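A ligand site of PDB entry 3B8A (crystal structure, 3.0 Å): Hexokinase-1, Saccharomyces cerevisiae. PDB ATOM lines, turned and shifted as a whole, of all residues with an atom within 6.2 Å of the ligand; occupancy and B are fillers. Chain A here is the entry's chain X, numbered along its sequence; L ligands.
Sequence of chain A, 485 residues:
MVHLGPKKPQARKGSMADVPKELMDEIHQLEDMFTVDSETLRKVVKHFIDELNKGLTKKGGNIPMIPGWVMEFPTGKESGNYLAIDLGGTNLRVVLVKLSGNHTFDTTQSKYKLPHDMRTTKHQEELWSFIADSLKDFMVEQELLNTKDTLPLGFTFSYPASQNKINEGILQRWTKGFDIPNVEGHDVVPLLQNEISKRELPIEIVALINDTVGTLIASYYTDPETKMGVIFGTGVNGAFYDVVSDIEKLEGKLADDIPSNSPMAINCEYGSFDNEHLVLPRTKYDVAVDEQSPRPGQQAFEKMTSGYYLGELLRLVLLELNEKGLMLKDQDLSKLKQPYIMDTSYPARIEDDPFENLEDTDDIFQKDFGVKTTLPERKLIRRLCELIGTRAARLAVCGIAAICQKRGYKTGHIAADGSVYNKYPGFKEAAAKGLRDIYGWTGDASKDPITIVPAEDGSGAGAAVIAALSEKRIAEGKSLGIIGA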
ATOM      1  N   PHE A 157     -16.045 -25.344 -15.994  1.00  0.00           N
ATOM      2  CA  PHE A 157     -16.456 -25.076 -14.624  1.00  0.00           C
ATOM      3  C   PHE A 157     -15.211 -25.009 -13.734  1.00  0.00           C
ATOM      4  O   PHE A 157     -14.720 -26.034 -13.262  1.00  0.00           O
ATOM      5  CB  PHE A 157     -17.404 -26.172 -14.148  1.00  0.00           C
ATOM      6  CG  PHE A 157     -18.127 -25.869 -12.873  1.00  0.00           C
ATOM      7  CD1 PHE A 157     -17.841 -26.585 -11.715  1.00  0.00           C
ATOM      8  CD2 PHE A 157     -19.084 -24.876 -12.822  1.00  0.00           C
ATOM      9  CE1 PHE A 157     -18.505 -26.311 -10.542  1.00  0.00           C
ATOM     10  CE2 PHE A 157     -19.757 -24.593 -11.643  1.00  0.00           C
ATOM     11  CZ  PHE A 157     -19.464 -25.308 -10.508  1.00  0.00           C
ATOM     12  N   SER A 158     -14.690 -23.805 -13.525  1.00  0.00           N
ATOM     13  CA  SER A 158     -13.389 -23.649 -12.856  1.00  0.00           C
ATOM     14  C   SER A 158     -13.471 -23.560 -11.332  1.00  0.00           C
ATOM     15  O   SER A 158     -12.979 -22.606 -10.731  1.00  0.00           O
ATOM     16  CB  SER A 158     -12.632 -22.455 -13.430  1.00  0.00           C
ATOM     17  OG  SER A 158     -13.434 -21.283 -13.437  1.00  0.00           O
ATOM     18  N   TYR A 159     -14.083 -24.572 -10.734  1.00  0.00           N
ATOM     19  CA  TYR A 159     -14.174 -24.674  -9.277  1.00  0.00           C
ATOM     20  C   TYR A 159     -13.849 -26.111  -8.927  1.00  0.00           C
ATOM     21  O   TYR A 159     -14.026 -26.995  -9.764  1.00  0.00           O
ATOM     22  CB  TYR A 159     -15.591 -24.286  -8.815  1.00  0.00           C
ATOM     23  CG  TYR A 159     -15.999 -22.952  -9.370  1.00  0.00           C
ATOM     24  CD1 TYR A 159     -16.601 -22.854 -10.629  1.00  0.00           C
ATOM     25  CD2 TYR A 159     -15.757 -21.784  -8.673  1.00  0.00           C
ATOM     26  CE1 TYR A 159     -16.945 -21.633 -11.149  1.00  0.00           C
ATOM     27  CE2 TYR A 159     -16.101 -20.562  -9.193  1.00  0.00           C
ATOM     28  CZ  TYR A 159     -16.700 -20.487 -10.430  1.00  0.00           C
ATOM     29  OH  TYR A 159     -17.045 -19.266 -10.950  1.00  0.00           O
ATOM     30  N   PRO A 160     -13.344 -26.351  -7.710  1.00  0.00           N
ATOM     31  CA  PRO A 160     -12.995 -27.726  -7.329  1.00  0.00           C
ATOM     32  C   PRO A 160     -14.154 -28.684  -7.587  1.00  0.00           C
ATOM     33  O   PRO A 160     -15.280 -28.454  -7.138  1.00  0.00           O
ATOM     34  CB  PRO A 160     -12.728 -27.612  -5.830  1.00  0.00           C
ATOM     35  CG  PRO A 160     -12.260 -26.232  -5.648  1.00  0.00           C
ATOM     36  CD  PRO A 160     -13.021 -25.392  -6.644  1.00  0.00           C
ATOM     37  N   ARG A 173     -16.235 -27.518  -3.420  1.00  0.00           N
ATOM     38  CA  ARG A 173     -16.466 -26.316  -2.643  1.00  0.00           C
ATOM     39  C   ARG A 173     -16.430 -25.089  -3.542  1.00  0.00           C
ATOM     40  O   ARG A 173     -15.684 -25.059  -4.529  1.00  0.00           O
ATOM     41  CB  ARG A 173     -15.427 -26.195  -1.531  1.00  0.00           C
ATOM     42  CG  ARG A 173     -14.018 -26.561  -1.969  1.00  0.00           C
ATOM     43  CD  ARG A 173     -13.136 -26.959  -0.798  1.00  0.00           C
ATOM     44  NE  ARG A 173     -12.069 -27.855  -1.219  1.00  0.00           N
ATOM     45  CZ  ARG A 173     -11.010 -27.488  -1.935  1.00  0.00           C
ATOM     46  NH1 ARG A 173     -10.866 -26.224  -2.314  1.00  0.00           N
ATOM     47  NH2 ARG A 173     -10.084 -28.390  -2.265  1.00  0.00           N
ATOM     48  N   THR A 175     -15.475 -21.284  -4.593  1.00  0.00           N
ATOM     49  CA  THR A 175     -14.370 -20.365  -4.361  1.00  0.00           C
ATOM     50  C   THR A 175     -14.578 -19.102  -5.192  1.00  0.00           C
ATOM     51  O   THR A 175     -15.581 -18.987  -5.898  1.00  0.00           O
ATOM     52  CB  THR A 175     -13.002 -20.992  -4.706  1.00  0.00           C
ATOM     53  OG1 THR A 175     -12.955 -21.307  -6.096  1.00  0.00           O
ATOM     54  CG2 THR A 175     -12.745 -22.242  -3.885  1.00  0.00           C
ATOM     55  N   LYS A 176     -13.638 -18.171  -5.095  1.00  0.00           N
ATOM     56  CA  LYS A 176     -13.662 -16.954  -5.902  1.00  0.00           C
ATOM     57  C   LYS A 176     -14.940 -16.117  -5.751  1.00  0.00           C
ATOM     58  O   LYS A 176     -15.406 -15.503  -6.717  1.00  0.00           O
ATOM     59  CB  LYS A 176     -13.393 -17.295  -7.375  1.00  0.00           C
ATOM     60  CG  LYS A 176     -11.976 -17.763  -7.641  1.00  0.00           C
ATOM     61  CD  LYS A 176     -11.941 -18.969  -8.558  1.00  0.00           C
ATOM     62  CE  LYS A 176     -12.591 -18.676  -9.902  1.00  0.00           C
ATOM     63  NZ  LYS A 176     -12.574 -19.856 -10.804  1.00  0.00           N
ATOM     64  N   ASN A 210     -11.857 -28.041 -16.606  1.00  0.00           N
ATOM     65  CA  ASN A 210     -11.315 -27.003 -15.738  1.00  0.00           C
ATOM     66  C   ASN A 210     -10.556 -25.965 -16.555  1.00  0.00           C
ATOM     67  O   ASN A 210      -9.814 -26.308 -17.477  1.00  0.00           O
ATOM     68  CB  ASN A 210     -10.385 -27.604 -14.680  1.00  0.00           C
ATOM     69  CG  ASN A 210      -9.974 -26.596 -13.631  1.00  0.00           C
ATOM     70  OD1 ASN A 210      -8.820 -26.175 -13.578  1.00  0.00           O
ATOM     71  ND2 ASN A 210     -10.914 -26.206 -12.776  1.00  0.00           N
ATOM     72  N   ASP A 211     -10.725 -24.688 -16.211  1.00  0.00           N
ATOM     73  CA  ASP A 211     -10.109 -23.597 -16.961  1.00  0.00           C
ATOM     74  C   ASP A 211      -8.598 -23.776 -17.208  1.00  0.00           C
ATOM     75  O   ASP A 211      -8.101 -23.424 -18.281  1.00  0.00           O
ATOM     76  CB  ASP A 211     -10.405 -22.232 -16.317  1.00  0.00           C
ATOM     77  CG  ASP A 211      -9.857 -22.100 -14.907  1.00  0.00           C
ATOM     78  OD1 ASP A 211      -9.521 -23.131 -14.297  1.00  0.00           O
ATOM     79  OD2 ASP A 211      -9.768 -20.962 -14.414  1.00  0.00           O
ATOM     80  N   THR A 212      -7.879 -24.329 -16.238  1.00  0.00           N
ATOM     81  CA  THR A 212      -6.439 -24.558 -16.402  1.00  0.00           C
ATOM     82  C   THR A 212      -6.174 -25.656 -17.423  1.00  0.00           C
ATOM     83  O   THR A 212      -5.164 -25.633 -18.123  1.00  0.00           O
ATOM     84  CB  THR A 212      -5.739 -24.918 -15.065  1.00  0.00           C
ATOM     85  OG1 THR A 212      -6.262 -26.147 -14.558  1.00  0.00           O
ATOM     86  CG2 THR A 212      -5.934 -23.839 -14.038  1.00  0.00           C
ATOM     87  N   ILE A 231      -3.014 -20.675 -14.312  1.00  0.00           N
ATOM     88  CA  ILE A 231      -3.877 -19.510 -14.145  1.00  0.00           C
ATOM     89  C   ILE A 231      -3.432 -18.675 -12.965  1.00  0.00           C
ATOM     90  O   ILE A 231      -3.458 -19.116 -11.820  1.00  0.00           O
ATOM     91  CB  ILE A 231      -5.345 -19.913 -13.938  1.00  0.00           C
ATOM     92  CG1 ILE A 231      -5.863 -20.697 -15.141  1.00  0.00           C
ATOM     93  CG2 ILE A 231      -6.201 -18.664 -13.717  1.00  0.00           C
ATOM     94  CD1 ILE A 231      -6.192 -19.837 -16.332  1.00  0.00           C
ATOM     95  N   GLY A 233      -5.024 -15.883 -11.719  1.00  0.00           N
ATOM     96  CA  GLY A 233      -6.214 -15.056 -11.776  1.00  0.00           C
ATOM     97  C   GLY A 233      -6.808 -14.760 -10.417  1.00  0.00           C
ATOM     98  O   GLY A 233      -6.084 -14.656  -9.427  1.00  0.00           O
ATOM     99  N   THR A 234      -8.129 -14.628 -10.362  1.00  0.00           N
ATOM    100  CA  THR A 234      -8.845 -14.463  -9.105  1.00  0.00           C
ATOM    101  C   THR A 234      -8.690 -15.734  -8.296  1.00  0.00           C
ATOM    102  O   THR A 234      -9.043 -15.789  -7.115  1.00  0.00           O
ATOM    103  CB  THR A 234     -10.339 -14.166  -9.343  1.00  0.00           C
ATOM    104  OG1 THR A 234     -10.463 -13.051 -10.227  1.00  0.00           O
ATOM    105  CG2 THR A 234     -11.059 -13.868  -8.037  1.00  0.00           C
ATOM    106  N   GLY A 235      -8.172 -16.761  -8.943  1.00  0.00           N
ATOM    107  CA  GLY A 235      -7.793 -17.994  -8.297  1.00  0.00           C
ATOM    108  C   GLY A 235      -6.520 -18.484  -8.957  1.00  0.00           C
ATOM    109  O   GLY A 235      -6.185 -18.037 -10.041  1.00  0.00           O
ATOM    110  N   VAL A 236      -5.807 -19.393  -8.300  1.00  0.00           N
ATOM    111  CA  VAL A 236      -4.608 -19.950  -8.908  1.00  0.00           C
ATOM    112  C   VAL A 236      -4.716 -21.473  -9.011  1.00  0.00           C
ATOM    113  O   VAL A 236      -5.276 -22.133  -8.141  1.00  0.00           O
ATOM    114  CB  VAL A 236      -3.306 -19.554  -8.156  1.00  0.00           C
ATOM    115  CG1 VAL A 236      -3.114 -18.052  -8.198  1.00  0.00           C
ATOM    116  CG2 VAL A 236      -3.331 -20.055  -6.725  1.00  0.00           C
ATOM    117  N   ASN A 237      -4.164 -21.998 -10.101  1.00  0.00           N
ATOM    118  CA  ASN A 237      -4.223 -23.410 -10.401  1.00  0.00           C
ATOM    119  C   ASN A 237      -3.331 -23.702 -11.608  1.00  0.00           C
ATOM    120  O   ASN A 237      -2.967 -22.793 -12.348  1.00  0.00           O
ATOM    121  CB  ASN A 237      -5.663 -23.824 -10.670  1.00  0.00           C
ATOM    122  CG  ASN A 237      -5.864 -25.318 -10.622  1.00  0.00           C
ATOM    123  OD1 ASN A 237      -6.923 -25.827 -10.994  1.00  0.00           O
ATOM    124  ND2 ASN A 237      -4.851 -26.050 -10.166  1.00  0.00           N
ATOM    125  N   GLY A 238      -2.984 -24.970 -11.797  1.00  0.00           N
ATOM    126  CA  GLY A 238      -2.142 -25.359 -12.902  1.00  0.00           C
ATOM    127  C   GLY A 238      -2.471 -26.764 -13.374  1.00  0.00           C
ATOM    128  O   GLY A 238      -2.718 -27.657 -12.570  1.00  0.00           O
ATOM    129  N   ASN A 267      -5.644 -31.893 -13.594  1.00  0.00           N
ATOM    130  CA  ASN A 267      -6.028 -30.657 -12.929  1.00  0.00           C
ATOM    131  C   ASN A 267      -5.537 -30.710 -11.486  1.00  0.00           C
ATOM    132  O   ASN A 267      -6.188 -31.292 -10.622  1.00  0.00           O
ATOM    133  CB  ASN A 267      -7.540 -30.482 -12.957  1.00  0.00           C
ATOM    134  CG  ASN A 267      -8.004 -29.330 -12.101  1.00  0.00           C
ATOM    135  OD1 ASN A 267      -9.157 -29.264 -11.702  1.00  0.00           O
ATOM    136  ND2 ASN A 267      -7.103 -28.412 -11.802  1.00  0.00           N
ATOM    137  N   GLU A 269      -5.302 -28.641  -8.968  1.00  0.00           N
ATOM    138  CA  GLU A 269      -6.013 -27.985  -7.871  1.00  0.00           C
ATOM    139  C   GLU A 269      -5.069 -27.712  -6.714  1.00  0.00           C
ATOM    140  O   GLU A 269      -5.405 -27.972  -5.553  1.00  0.00           O
ATOM    141  CB  GLU A 269      -7.192 -28.838  -7.400  1.00  0.00           C
ATOM    142  CG  GLU A 269      -8.424 -28.735  -8.270  1.00  0.00           C
ATOM    143  CD  GLU A 269      -9.095 -27.377  -8.193  1.00  0.00           C
ATOM    144  OE1 GLU A 269      -8.843 -26.649  -7.218  1.00  0.00           O
ATOM    145  OE2 GLU A 269      -9.879 -27.040  -9.111  1.00  0.00           O
ATOM    146  N   GLN A 299      -7.157 -23.694   1.028  1.00  0.00           N
ATOM    147  CA  GLN A 299      -6.480 -22.871   0.027  1.00  0.00           C
ATOM    148  C   GLN A 299      -5.326 -22.059   0.606  1.00  0.00           C
ATOM    149  O   GLN A 299      -5.255 -20.851   0.387  1.00  0.00           O
ATOM    150  CB  GLN A 299      -7.484 -21.925  -0.624  1.00  0.00           C
ATOM    151  CG  GLN A 299      -8.863 -22.521  -0.792  1.00  0.00           C
ATOM    152  CD  GLN A 299      -9.899 -21.477  -1.194  1.00  0.00           C
ATOM    153  OE1 GLN A 299      -9.965 -21.071  -2.348  1.00  0.00           O
ATOM    154  NE2 GLN A 299     -10.706 -21.055  -0.222  1.00  0.00           N
ATOM    155  N   GLU A 302      -3.220 -20.686  -2.237  1.00  0.00           N
ATOM    156  CA  GLU A 302      -4.028 -19.751  -3.018  1.00  0.00           C
ATOM    157  C   GLU A 302      -4.301 -18.446  -2.261  1.00  0.00           C
ATOM    158  O   GLU A 302      -4.260 -17.365  -2.840  1.00  0.00           O
ATOM    159  CB  GLU A 302      -5.341 -20.414  -3.410  1.00  0.00           C
ATOM    160  CG  GLU A 302      -6.228 -19.554  -4.278  1.00  0.00           C
ATOM    161  CD  GLU A 302      -7.397 -20.331  -4.815  1.00  0.00           C
ATOM    162  OE1 GLU A 302      -7.765 -21.358  -4.194  1.00  0.00           O
ATOM    163  OE2 GLU A 302      -7.963 -19.934  -5.851  1.00  0.00           O
HETATM  164  C1  LIG L   1     -10.291 -23.143  -8.600  1.00  0.00           C
HETATM  165  C2  LIG L   1      -9.714 -23.849  -9.823  1.00  0.00           C
HETATM  166  C3  LIG L   1      -9.391 -22.865 -10.939  1.00  0.00           C
HETATM  167  C4  LIG L   1      -8.655 -21.633 -10.421  1.00  0.00           C
HETATM  168  C5  LIG L   1      -8.472 -20.608 -11.534  1.00  0.00           C
HETATM  169  C6  LIG L   1      -9.462 -21.912  -8.241  1.00  0.00           C
HETATM  170  O1  LIG L   1     -10.056 -21.225  -7.174  1.00  0.00           O
HETATM  171  O2  LIG L   1     -10.314 -24.021  -7.506  1.00  0.00           O
HETATM  172  O3  LIG L   1     -10.647 -24.790 -10.312  1.00  0.00           O
HETATM  173  O4  LIG L   1      -8.562 -23.507 -11.882  1.00  0.00           O
HETATM  174  O5  LIG L   1      -9.381 -21.056  -9.365  1.00  0.00           O
HETATM  175  O6  LIG L   1      -9.706 -19.986 -11.798  1.00  0.00           O
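ND2 of Asn 210 is in hydrogen-bond range of O3 of the ligand, at 2.9 Å. OG1 of Thr 175 lies within hydrogen-bond range of O1 of the ligand (3.1 Å). NZ of Lys 176 is in hydrogen-bond range of O6 of the ligand (3.0 Å). The side-chain carboxylate (OE2) of Glu 302 is in hydrogen-bond range of an oxygen (O1) of the ligand (2.8 Å). The side-chain amide oxygen of Asn 237 sits at hydrogen-bond distance from an oxygen (O4) of the ligand (3.0 Å). O3 of the ligand sits at hydrogen-bond distance from OE2 of Glu 269 (2.7 Å). An oxygen (O4) of the ligand is in hydrogen-bond range of the side-chain carboxylate (OD1) of Asp 211. N of Tyr 159 lies within hydrogen-bond range of O3 of the ligand (3.5 Å). The backbone carbonyl oxygen (O) of Ser 158 sits at hydrogen-bond distance from an oxygen (O3) of the ligand, 3.2 Å away.
CD of Pro 160 touches O2 of the ligand (3.2 Å). Thr 212 touches the ligand. Ile 231 touches the ligand. Gly 235 touches the ligand (CA to O5, 3.6 Å). Hydrophobic or aromatic side chains within 4 Å of the ligand: Pro 160 and Ile 231.
The side-chain amide oxygen (OD1) of Asn 210 lies within hydrogen-bond range of the side-chain hydroxyl (OG1) of Thr 212, at 2.7 Å. The side-chain amide oxygen of Asn 210 sits close to the side-chain carboxylate of Asp 211. The side-chain amide oxygen of Asn 237 sits at hydrogen-bond distance from the side-chain amide nitrogen of Asn 267 (2.7 Å). The side-chain amide oxygen (OD1) of Asn 210 sits close to the side-chain amide oxygen (OD1) of Asn 237, at 3.2 Å. N of Ile 231 is in hydrogen-bond range of O of Asn 237. OE1 of Glu 302 lies close to OE1 of Gln 299, 2.9 Å away. The side-chain amide nitrogen (ND2) of Asn 267 sits close to the backbone NH (N) of Glu 269, 3.4 Å away. The side-chain amide oxygen of Asn 210 lies within hydrogen-bond range of the side-chain amide nitrogen of Asn 267 (3.3 Å).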
